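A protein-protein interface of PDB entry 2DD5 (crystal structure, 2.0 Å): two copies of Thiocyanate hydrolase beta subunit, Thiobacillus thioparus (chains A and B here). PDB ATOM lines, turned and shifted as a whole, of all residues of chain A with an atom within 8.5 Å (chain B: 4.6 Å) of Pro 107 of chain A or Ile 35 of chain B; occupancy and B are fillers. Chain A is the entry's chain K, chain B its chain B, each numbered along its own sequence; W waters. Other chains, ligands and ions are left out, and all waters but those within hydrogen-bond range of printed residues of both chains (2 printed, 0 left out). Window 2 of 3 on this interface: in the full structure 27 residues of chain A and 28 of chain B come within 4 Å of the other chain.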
ATOM      1  N   LYS A  63      18.848  23.859  -1.187  1.00  0.00           N
ATOM      2  CA  LYS A  63      18.882  24.625   0.052  1.00  0.00           C
ATOM      3  C   LYS A  63      19.185  26.073  -0.274  1.00  0.00           C
ATOM      4  O   LYS A  63      20.094  26.358  -1.054  1.00  0.00           O
ATOM      5  CB  LYS A  63      19.947  24.113   1.027  1.00  0.00           C
ATOM      6  CG  LYS A  63      19.883  24.821   2.395  1.00  0.00           C
ATOM      7  CD  LYS A  63      21.022  24.419   3.335  1.00  0.00           C
ATOM      8  CE  LYS A  63      22.292  25.222   3.076  1.00  0.00           C
ATOM      9  NZ  LYS A  63      22.110  26.678   3.394  1.00  0.00           N
ATOM     10  N   TRP A  68      25.331  34.474   5.512  1.00  0.00           N
ATOM     11  CA  TRP A  68      26.679  34.233   6.019  1.00  0.00           C
ATOM     12  C   TRP A  68      27.479  33.280   5.133  1.00  0.00           C
ATOM     13  O   TRP A  68      28.707  33.375   5.068  1.00  0.00           O
ATOM     14  CB  TRP A  68      26.666  33.739   7.480  1.00  0.00           C
ATOM     15  CG  TRP A  68      26.207  32.315   7.734  1.00  0.00           C
ATOM     16  CD1 TRP A  68      24.968  31.916   8.145  1.00  0.00           C
ATOM     17  CD2 TRP A  68      27.005  31.125   7.654  1.00  0.00           C
ATOM     18  NE1 TRP A  68      24.944  30.548   8.331  1.00  0.00           N
ATOM     19  CE2 TRP A  68      26.181  30.040   8.035  1.00  0.00           C
ATOM     20  CE3 TRP A  68      28.337  30.868   7.298  1.00  0.00           C
ATOM     21  CZ2 TRP A  68      26.645  28.717   8.069  1.00  0.00           C
ATOM     22  CZ3 TRP A  68      28.799  29.553   7.333  1.00  0.00           C
ATOM     23  CH2 TRP A  68      27.953  28.497   7.716  1.00  0.00           C
ATOM     24  N   GLU A  69      26.790  32.377   4.439  1.00  0.00           N
ATOM     25  CA  GLU A  69      27.471  31.442   3.547  1.00  0.00           C
ATOM     26  C   GLU A  69      28.037  32.204   2.353  1.00  0.00           C
ATOM     27  O   GLU A  69      29.180  31.996   1.957  1.00  0.00           O
ATOM     28  CB  GLU A  69      26.506  30.343   3.077  1.00  0.00           C
ATOM     29  CG  GLU A  69      25.999  29.462   4.212  1.00  0.00           C
ATOM     30  CD  GLU A  69      25.071  28.369   3.735  1.00  0.00           C
ATOM     31  OE1 GLU A  69      24.225  28.652   2.857  1.00  0.00           O
ATOM     32  OE2 GLU A  69      25.181  27.230   4.245  1.00  0.00           O
ATOM     33  N   GLN A  94      40.574  22.577   4.883  1.00  0.00           N
ATOM     34  CA  GLN A  94      39.126  22.539   5.024  1.00  0.00           C
ATOM     35  C   GLN A  94      38.433  21.182   4.936  1.00  0.00           C
ATOM     36  O   GLN A  94      37.516  20.890   5.715  1.00  0.00           O
ATOM     37  CB  GLN A  94      38.536  23.478   3.974  1.00  0.00           C
ATOM     38  CG  GLN A  94      37.030  23.536   3.910  1.00  0.00           C
ATOM     39  CD  GLN A  94      36.572  24.206   2.633  1.00  0.00           C
ATOM     40  OE1 GLN A  94      36.858  25.381   2.403  1.00  0.00           O
ATOM     41  NE2 GLN A  94      35.879  23.452   1.781  1.00  0.00           N
ATOM     42  N   ASN A  95      38.865  20.356   3.993  1.00  0.00           N
ATOM     43  CA  ASN A  95      38.232  19.067   3.778  1.00  0.00           C
ATOM     44  C   ASN A  95      38.993  17.870   4.325  1.00  0.00           C
ATOM     45  O   ASN A  95      38.497  16.742   4.272  1.00  0.00           O
ATOM     46  CB  ASN A  95      37.990  18.868   2.279  1.00  0.00           C
ATOM     47  CG  ASN A  95      37.294  20.053   1.639  1.00  0.00           C
ATOM     48  OD1 ASN A  95      36.366  20.616   2.210  1.00  0.00           O
ATOM     49  ND2 ASN A  95      37.735  20.431   0.440  1.00  0.00           N
ATOM     50  N   THR A 101      35.459  13.621  12.476  1.00  0.00           N
ATOM     51  CA  THR A 101      34.292  14.066  13.236  1.00  0.00           C
ATOM     52  C   THR A 101      33.704  15.388  12.761  1.00  0.00           C
ATOM     53  O   THR A 101      32.506  15.481  12.498  1.00  0.00           O
ATOM     54  CB  THR A 101      34.614  14.173  14.741  1.00  0.00           C
ATOM     55  OG1 THR A 101      34.950  12.874  15.244  1.00  0.00           O
ATOM     56  CG2 THR A 101      33.410  14.721  15.515  1.00  0.00           C
ATOM     57  N   VAL A 102      34.537  16.417  12.662  1.00  0.00           N
ATOM     58  CA  VAL A 102      34.047  17.712  12.207  1.00  0.00           C
ATOM     59  C   VAL A 102      33.678  17.655  10.723  1.00  0.00           C
ATOM     60  O   VAL A 102      32.735  18.313  10.283  1.00  0.00           O
ATOM     61  CB  VAL A 102      35.098  18.819  12.421  1.00  0.00           C
ATOM     62  CG1 VAL A 102      34.698  20.084  11.654  1.00  0.00           C
ATOM     63  CG2 VAL A 102      35.219  19.135  13.914  1.00  0.00           C
ATOM     64  N   TYR A 103      34.422  16.863   9.957  1.00  0.00           N
ATOM     65  CA  TYR A 103      34.173  16.741   8.528  1.00  0.00           C
ATOM     66  C   TYR A 103      32.730  16.362   8.198  1.00  0.00           C
ATOM     67  O   TYR A 103      32.131  16.921   7.278  1.00  0.00           O
ATOM     68  CB  TYR A 103      35.124  15.713   7.906  1.00  0.00           C
ATOM     69  CG  TYR A 103      35.017  15.667   6.397  1.00  0.00           C
ATOM     70  CD1 TYR A 103      35.322  16.793   5.627  1.00  0.00           C
ATOM     71  CD2 TYR A 103      34.555  14.523   5.742  1.00  0.00           C
ATOM     72  CE1 TYR A 103      35.165  16.787   4.244  1.00  0.00           C
ATOM     73  CE2 TYR A 103      34.391  14.506   4.347  1.00  0.00           C
ATOM     74  CZ  TYR A 103      34.696  15.641   3.610  1.00  0.00           C
ATOM     75  OH  TYR A 103      34.515  15.655   2.244  1.00  0.00           O
ATOM     76  N   LEU A 104      32.160  15.426   8.948  1.00  0.00           N
ATOM     77  CA  LEU A 104      30.788  15.001   8.686  1.00  0.00           C
ATOM     78  C   LEU A 104      29.771  15.521   9.701  1.00  0.00           C
ATOM     79  O   LEU A 104      28.563  15.476   9.457  1.00  0.00           O
ATOM     80  CB  LEU A 104      30.731  13.471   8.603  1.00  0.00           C
ATOM     81  CG  LEU A 104      31.426  12.896   7.360  1.00  0.00           C
ATOM     82  CD1 LEU A 104      31.518  11.376   7.450  1.00  0.00           C
ATOM     83  CD2 LEU A 104      30.634  13.304   6.118  1.00  0.00           C
ATOM     84  N   GLY A 105      30.255  16.033  10.828  1.00  0.00           N
ATOM     85  CA  GLY A 105      29.346  16.541  11.844  1.00  0.00           C
ATOM     86  C   GLY A 105      28.896  17.976  11.636  1.00  0.00           C
ATOM     87  O   GLY A 105      27.771  18.340  11.985  1.00  0.00           O
ATOM     88  N   MET A 106      29.768  18.800  11.069  1.00  0.00           N
ATOM     89  CA  MET A 106      29.444  20.206  10.841  1.00  0.00           C
ATOM     90  C   MET A 106      28.979  20.445   9.409  1.00  0.00           C
ATOM     91  O   MET A 106      29.179  19.602   8.543  1.00  0.00           O
ATOM     92  CB  MET A 106      30.666  21.072  11.148  1.00  0.00           C
ATOM     93  CG  MET A 106      30.962  21.196  12.642  1.00  0.00           C
ATOM     94  SD  MET A 106      29.764  22.287  13.477  1.00  0.00           S
ATOM     95  CE  MET A 106      30.575  23.859  13.224  1.00  0.00           C
ATOM     96  N   PRO A 107      28.342  21.598   9.151  1.00  0.00           N
ATOM     97  CA  PRO A 107      27.849  21.937   7.815  1.00  0.00           C
ATOM     98  C   PRO A 107      28.972  22.270   6.849  1.00  0.00           C
ATOM     99  O   PRO A 107      30.050  22.731   7.247  1.00  0.00           O
ATOM    100  CB  PRO A 107      26.963  23.163   8.058  1.00  0.00           C
ATOM    101  CG  PRO A 107      26.629  23.097   9.522  1.00  0.00           C
ATOM    102  CD  PRO A 107      27.909  22.607  10.131  1.00  0.00           C
ATOM    103  N   TYR A 108      28.686  22.037   5.576  1.00  0.00           N
ATOM    104  CA  TYR A 108      29.594  22.319   4.469  1.00  0.00           C
ATOM    105  C   TYR A 108      30.259  23.693   4.648  1.00  0.00           C
ATOM    106  O   TYR A 108      31.477  23.790   4.809  1.00  0.00           O
ATOM    107  CB  TYR A 108      28.767  22.280   3.179  1.00  0.00           C
ATOM    108  CG  TYR A 108      29.446  22.741   1.909  1.00  0.00           C
ATOM    109  CD1 TYR A 108      30.207  21.861   1.134  1.00  0.00           C
ATOM    110  CD2 TYR A 108      29.249  24.036   1.433  1.00  0.00           C
ATOM    111  CE1 TYR A 108      30.740  22.265  -0.098  1.00  0.00           C
ATOM    112  CE2 TYR A 108      29.780  24.450   0.210  1.00  0.00           C
ATOM    113  CZ  TYR A 108      30.516  23.565  -0.551  1.00  0.00           C
ATOM    114  OH  TYR A 108      30.997  23.979  -1.777  1.00  0.00           O
ATOM    115  N   TYR A 109      29.460  24.756   4.636  1.00  0.00           N
ATOM    116  CA  TYR A 109      30.028  26.093   4.771  1.00  0.00           C
ATOM    117  C   TYR A 109      30.570  26.407   6.164  1.00  0.00           C
ATOM    118  O   TYR A 109      31.312  27.371   6.339  1.00  0.00           O
ATOM    119  CB  TYR A 109      29.017  27.152   4.314  1.00  0.00           C
ATOM    120  CG  TYR A 109      29.178  27.515   2.844  1.00  0.00           C
ATOM    121  CD1 TYR A 109      28.091  27.493   1.969  1.00  0.00           C
ATOM    122  CD2 TYR A 109      30.421  27.898   2.336  1.00  0.00           C
ATOM    123  CE1 TYR A 109      28.239  27.848   0.622  1.00  0.00           C
ATOM    124  CE2 TYR A 109      30.581  28.254   0.990  1.00  0.00           C
ATOM    125  CZ  TYR A 109      29.487  28.226   0.144  1.00  0.00           C
ATOM    126  OH  TYR A 109      29.642  28.571  -1.182  1.00  0.00           O
ATOM    127  N   GLY A 110      30.212  25.589   7.151  1.00  0.00           N
ATOM    128  CA  GLY A 110      30.738  25.793   8.488  1.00  0.00           C
ATOM    129  C   GLY A 110      32.226  25.486   8.439  1.00  0.00           C
ATOM    130  O   GLY A 110      33.040  26.153   9.078  1.00  0.00           O
ATOM    131  N   ARG A 111      32.586  24.464   7.667  1.00  0.00           N
ATOM    132  CA  ARG A 111      33.987  24.087   7.522  1.00  0.00           C
ATOM    133  C   ARG A 111      34.736  25.142   6.707  1.00  0.00           C
ATOM    134  O   ARG A 111      35.897  25.428   6.986  1.00  0.00           O
ATOM    135  CB  ARG A 111      34.109  22.706   6.865  1.00  0.00           C
ATOM    136  CG  ARG A 111      33.522  21.584   7.716  1.00  0.00           C
ATOM    137  CD  ARG A 111      33.729  20.203   7.101  1.00  0.00           C
ATOM    138  NE  ARG A 111      33.009  20.032   5.838  1.00  0.00           N
ATOM    139  CZ  ARG A 111      33.558  20.153   4.632  1.00  0.00           C
ATOM    140  NH1 ARG A 111      34.844  20.449   4.509  1.00  0.00           N
ATOM    141  NH2 ARG A 111      32.817  19.968   3.543  1.00  0.00           N
ATOM    142  N   TRP A 112      34.084  25.716   5.698  1.00  0.00           N
ATOM    143  CA  TRP A 112      34.729  26.766   4.906  1.00  0.00           C
ATOM    144  C   TRP A 112      35.084  27.940   5.834  1.00  0.00           C
ATOM    145  O   TRP A 112      36.200  28.463   5.799  1.00  0.00           O
ATOM    146  CB  TRP A 112      33.797  27.301   3.803  1.00  0.00           C
ATOM    147  CG  TRP A 112      33.678  26.462   2.547  1.00  0.00           C
ATOM    148  CD1 TRP A 112      33.098  25.228   2.429  1.00  0.00           C
ATOM    149  CD2 TRP A 112      34.119  26.827   1.227  1.00  0.00           C
ATOM    150  NE1 TRP A 112      33.149  24.804   1.117  1.00  0.00           N
ATOM    151  CE2 TRP A 112      33.767  25.765   0.360  1.00  0.00           C
ATOM    152  CE3 TRP A 112      34.774  27.947   0.695  1.00  0.00           C
ATOM    153  CZ2 TRP A 112      34.052  25.789  -1.017  1.00  0.00           C
ATOM    154  CZ3 TRP A 112      35.057  27.973  -0.676  1.00  0.00           C
ATOM    155  CH2 TRP A 112      34.693  26.897  -1.513  1.00  0.00           C
ATOM    156  N   LEU A 113      34.124  28.343   6.665  1.00  0.00           N
ATOM    157  CA  LEU A 113      34.310  29.468   7.580  1.00  0.00           C
ATOM    158  C   LEU A 113      35.364  29.214   8.649  1.00  0.00           C
ATOM    159  O   LEU A 113      36.233  30.055   8.885  1.00  0.00           O
ATOM    160  CB  LEU A 113      32.979  29.831   8.243  1.00  0.00           C
ATOM    161  CG  LEU A 113      32.999  30.976   9.266  1.00  0.00           C
ATOM    162  CD1 LEU A 113      33.594  32.243   8.648  1.00  0.00           C
ATOM    163  CD2 LEU A 113      31.573  31.225   9.739  1.00  0.00           C
ATOM    164  N   LEU A 114      35.279  28.066   9.308  1.00  0.00           N
ATOM    165  CA  LEU A 114      36.253  27.716  10.333  1.00  0.00           C
ATOM    166  C   LEU A 114      37.661  27.743   9.755  1.00  0.00           C
ATOM    167  O   LEU A 114      38.607  28.194  10.409  1.00  0.00           O
ATOM    168  CB  LEU A 114      35.970  26.314  10.878  1.00  0.00           C
ATOM    169  CG  LEU A 114      34.775  26.182  11.828  1.00  0.00           C
ATOM    170  CD1 LEU A 114      34.449  24.707  12.046  1.00  0.00           C
ATOM    171  CD2 LEU A 114      35.107  26.871  13.154  1.00  0.00           C
ATOM    172  N   PRO B  30      25.182  17.984   8.147  1.00  0.00           N
ATOM    173  CA  PRO B  30      23.864  18.599   8.314  1.00  0.00           C
ATOM    174  C   PRO B  30      23.877  20.081   7.937  1.00  0.00           C
ATOM    175  O   PRO B  30      24.932  20.713   7.902  1.00  0.00           O
ATOM    176  CB  PRO B  30      23.574  18.385   9.799  1.00  0.00           C
ATOM    177  CG  PRO B  30      24.934  18.484  10.410  1.00  0.00           C
ATOM    178  CD  PRO B  30      25.775  17.651   9.456  1.00  0.00           C
ATOM    179  N   ALA B  31      22.701  20.624   7.644  1.00  0.00           N
ATOM    180  CA  ALA B  31      22.577  22.034   7.287  1.00  0.00           C
ATOM    181  C   ALA B  31      22.855  22.888   8.525  1.00  0.00           C
ATOM    182  O   ALA B  31      22.770  22.400   9.654  1.00  0.00           O
ATOM    183  CB  ALA B  31      21.166  22.311   6.756  1.00  0.00           C
ATOM    184  N   PRO B  32      23.195  24.174   8.329  1.00  0.00           N
ATOM    185  CA  PRO B  32      23.482  25.091   9.437  1.00  0.00           C
ATOM    186  C   PRO B  32      22.327  25.169  10.435  1.00  0.00           C
ATOM    187  O   PRO B  32      22.539  25.339  11.636  1.00  0.00           O
ATOM    188  CB  PRO B  32      23.713  26.422   8.726  1.00  0.00           C
ATOM    189  CG  PRO B  32      24.345  25.986   7.432  1.00  0.00           C
ATOM    190  CD  PRO B  32      23.456  24.826   7.033  1.00  0.00           C
ATOM    191  N   THR B  33      21.108  25.041   9.923  1.00  0.00           N
ATOM    192  CA  THR B  33      19.907  25.101  10.746  1.00  0.00           C
ATOM    193  C   THR B  33      19.747  23.916  11.703  1.00  0.00           C
ATOM    194  O   THR B  33      18.866  23.928  12.562  1.00  0.00           O
ATOM    195  CB  THR B  33      18.644  25.222   9.863  1.00  0.00           C
ATOM    196  OG1 THR B  33      18.728  24.299   8.766  1.00  0.00           O
ATOM    197  CG2 THR B  33      18.514  26.639   9.318  1.00  0.00           C
ATOM    198  N   GLU B  34      20.594  22.899  11.556  1.00  0.00           N
ATOM    199  CA  GLU B  34      20.540  21.734  12.437  1.00  0.00           C
ATOM    200  C   GLU B  34      21.625  21.807  13.505  1.00  0.00           C
ATOM    201  O   GLU B  34      21.762  20.903  14.333  1.00  0.00           O
ATOM    202  CB  GLU B  34      20.695  20.441  11.632  1.00  0.00           C
ATOM    203  CG  GLU B  34      19.504  20.132  10.736  1.00  0.00           C
ATOM    204  CD  GLU B  34      18.205  20.028  11.521  1.00  0.00           C
ATOM    205  OE1 GLU B  34      18.103  19.136  12.394  1.00  0.00           O
ATOM    206  OE2 GLU B  34      17.286  20.842  11.272  1.00  0.00           O
ATOM    207  N   ILE B  35      22.398  22.887  13.484  1.00  0.00           N
ATOM    208  CA  ILE B  35      23.470  23.076  14.450  1.00  0.00           C
ATOM    209  C   ILE B  35      23.055  24.093  15.508  1.00  0.00           C
ATOM    210  O   ILE B  35      22.956  25.287  15.229  1.00  0.00           O
ATOM    211  CB  ILE B  35      24.763  23.584  13.764  1.00  0.00           C
ATOM    212  CG1 ILE B  35      25.229  22.576  12.705  1.00  0.00           C
ATOM    213  CG2 ILE B  35      25.858  23.807  14.804  1.00  0.00           C
ATOM    214  CD1 ILE B  35      25.568  21.207  13.253  1.00  0.00           C
ATOM    215  N   THR B  36      22.795  23.609  16.718  1.00  0.00           N
ATOM    216  CA  THR B  36      22.410  24.478  17.827  1.00  0.00           C
ATOM    217  C   THR B  36      23.689  25.068  18.405  1.00  0.00           C
ATOM    218  O   THR B  36      24.788  24.660  18.034  1.00  0.00           O
ATOM    219  CB  THR B  36      21.730  23.682  18.947  1.00  0.00           C
ATOM    220  OG1 THR B  36      22.625  22.657  19.396  1.00  0.00           O
ATOM    221  CG2 THR B  36      20.436  23.045  18.456  1.00  0.00           C
ATOM    222  N   HIS B  37      23.553  26.021  19.319  1.00  0.00           N
ATOM    223  CA  HIS B  37      24.731  26.612  19.929  1.00  0.00           C
ATOM    224  C   HIS B  37      25.497  25.539  20.704  1.00  0.00           C
ATOM    225  O   HIS B  37      26.728  25.511  20.697  1.00  0.00           O
ATOM    226  CB  HIS B  37      24.342  27.756  20.869  1.00  0.00           C
ATOM    227  CG  HIS B  37      25.503  28.317  21.627  1.00  0.00           C
ATOM    228  ND1 HIS B  37      25.823  27.910  22.905  1.00  0.00           N
ATOM    229  CD2 HIS B  37      26.473  29.184  21.255  1.00  0.00           C
ATOM    230  CE1 HIS B  37      26.942  28.500  23.285  1.00  0.00           C
ATOM    231  NE2 HIS B  37      27.357  29.277  22.302  1.00  0.00           N
ATOM    232  N   LEU B  39      25.720  22.330  20.073  1.00  0.00           N
ATOM    233  CA  LEU B  39      26.479  21.492  19.149  1.00  0.00           C
ATOM    234  C   LEU B  39      27.649  22.259  18.551  1.00  0.00           C
ATOM    235  O   LEU B  39      28.721  21.692  18.343  1.00  0.00           O
ATOM    236  CB  LEU B  39      25.578  20.961  18.027  1.00  0.00           C
ATOM    237  CG  LEU B  39      24.564  19.885  18.425  1.00  0.00           C
ATOM    238  CD1 LEU B  39      23.707  19.518  17.223  1.00  0.00           C
ATOM    239  CD2 LEU B  39      25.300  18.659  18.955  1.00  0.00           C
ATOM    240  N   PHE B  40      27.448  23.546  18.270  1.00  0.00           N
ATOM    241  CA  PHE B  40      28.526  24.354  17.710  1.00  0.00           C
ATOM    242  C   PHE B  40      29.694  24.344  18.694  1.00  0.00           C
ATOM    243  O   PHE B  40      30.849  24.169  18.301  1.00  0.00           O
ATOM    244  CB  PHE B  40      28.070  25.797  17.471  1.00  0.00           C
ATOM    245  CG  PHE B  40      29.114  26.658  16.804  1.00  0.00           C
ATOM    246  CD1 PHE B  40      29.214  26.708  15.415  1.00  0.00           C
ATOM    247  CD2 PHE B  40      30.022  27.386  17.566  1.00  0.00           C
ATOM    248  CE1 PHE B  40      30.205  27.473  14.795  1.00  0.00           C
ATOM    249  CE2 PHE B  40      31.018  28.152  16.957  1.00  0.00           C
ATOM    250  CZ  PHE B  40      31.110  28.196  15.568  1.00  0.00           C
ATOM    251  N   TYR B  43      31.327  20.746  18.795  1.00  0.00           N
ATOM    252  CA  TYR B  43      32.145  20.437  17.622  1.00  0.00           C
ATOM    253  C   TYR B  43      33.423  21.259  17.536  1.00  0.00           C
ATOM    254  O   TYR B  43      34.431  20.781  17.015  1.00  0.00           O
ATOM    255  CB  TYR B  43      31.343  20.627  16.323  1.00  0.00           C
ATOM    256  CG  TYR B  43      30.421  19.474  15.988  1.00  0.00           C
ATOM    257  CD1 TYR B  43      29.051  19.675  15.823  1.00  0.00           C
ATOM    258  CD2 TYR B  43      30.920  18.179  15.832  1.00  0.00           C
ATOM    259  CE1 TYR B  43      28.200  18.615  15.515  1.00  0.00           C
ATOM    260  CE2 TYR B  43      30.078  17.115  15.523  1.00  0.00           C
ATOM    261  CZ  TYR B  43      28.722  17.340  15.368  1.00  0.00           C
ATOM    262  OH  TYR B  43      27.889  16.293  15.079  1.00  0.00           O
HETATM  263  O   HOH W   1      25.869  17.240  13.615  1.00  0.00           O
HETATM  264  O   HOH W   2      26.275  20.692   4.856  1.00  0.00           O
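The side-chain carboxylate (OE1) of Glu 69 of chain A is in salt-bridge range of the side-chain amino group (NZ) of Lys 63 of chain A.
CG of Pro 32 of chain B touches CZ2 of Trp 68 of chain A, at 3.6 Å. CG of Pro 32 of chain B touches OE2 of Glu 69 of chain A (3.5 Å). Val 102 of chain A touches Tyr 43 of chain B (CG2 to O, 3.6 Å). CD of Pro 30 of chain B touches O of Leu 104 of chain A, 3.5 Å away. Ile 35 of chain B touches Gly 105 of chain A. Gly 105 of chain A touches Tyr 43 of chain B. Phe 40 of chain B touches Met 106 of chain A. Pro 107 of chain A touches Ala 31 of chain B. Pro 107 of chain A touches Pro 32 of chain B (CG to CA, 3.7 Å). Pro 107 of chain A touches Ile 35 of chain B (CG to CG1, 3.5 Å).
Gln 94 of chain A touches none of the printed residues of chain B. Of the printed residues of chain B, Val 102 of chain A touches Tyr 43. Of the printed residues of chain B, Leu 104 of chain A touches Pro 30 (3.5 Å). Of the printed residues of chain B, Met 106 of chain A touches Phe 40 (3.8 Å) and Tyr 43 (3.6 Å). Of the printed residues of chain B, Pro 107 of chain A touches Pro 30 (3.2 Å), Ala 31 (3.9 Å), Pro 32 (3.7 Å) and Ile 35 (3.5 Å). Gly 110 of chain A touches none of the printed residues of chain B. Ile 35 of chain B touches two residues of chain A. No residue of chain A comes within 4 Å of Thr 36 of chain B. Of the printed residues of chain A, Tyr 43 of chain B touches Val 102 (3.6 Å), Gly 105 (3.6 Å) and Met 106 (3.6 Å). The nearest printed residue of chain B that does not touch Gly 105 of chain A is Leu 39 of chain B (6.7 Å).
Of the 19 printed residues of chain A, 7 touch a printed residue of chain B. Hydrophobic or aromatic side chains of chain A within 4 Å of the printed part of chain B: Trp 68, Val 102, Met 106 and Pro 107. Along chain A the printed residues that touch a printed residue of chain B span positions 68 to 107. Among the printed residues, 13 pairs touch across the chains. Among the printed residues, no Asp or Glu carboxylate lies within 4 Å of a Lys or Arg side-chain nitrogen of the other chain.
No position is printed for both chains.
Water W1 lies within hydrogen-bond range of the side-chain hydroxyl of Tyr 43 of chain B (2.7 Å) and the backbone carbonyl oxygen of Gly 105 of chain A (2.7 Å). Water W2 lies within hydrogen-bond range of the backbone NH of Tyr 108 of chain A (2.9 Å) and the backbone carbonyl oxygen of Pro 30 of chain B (3.3 Å).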
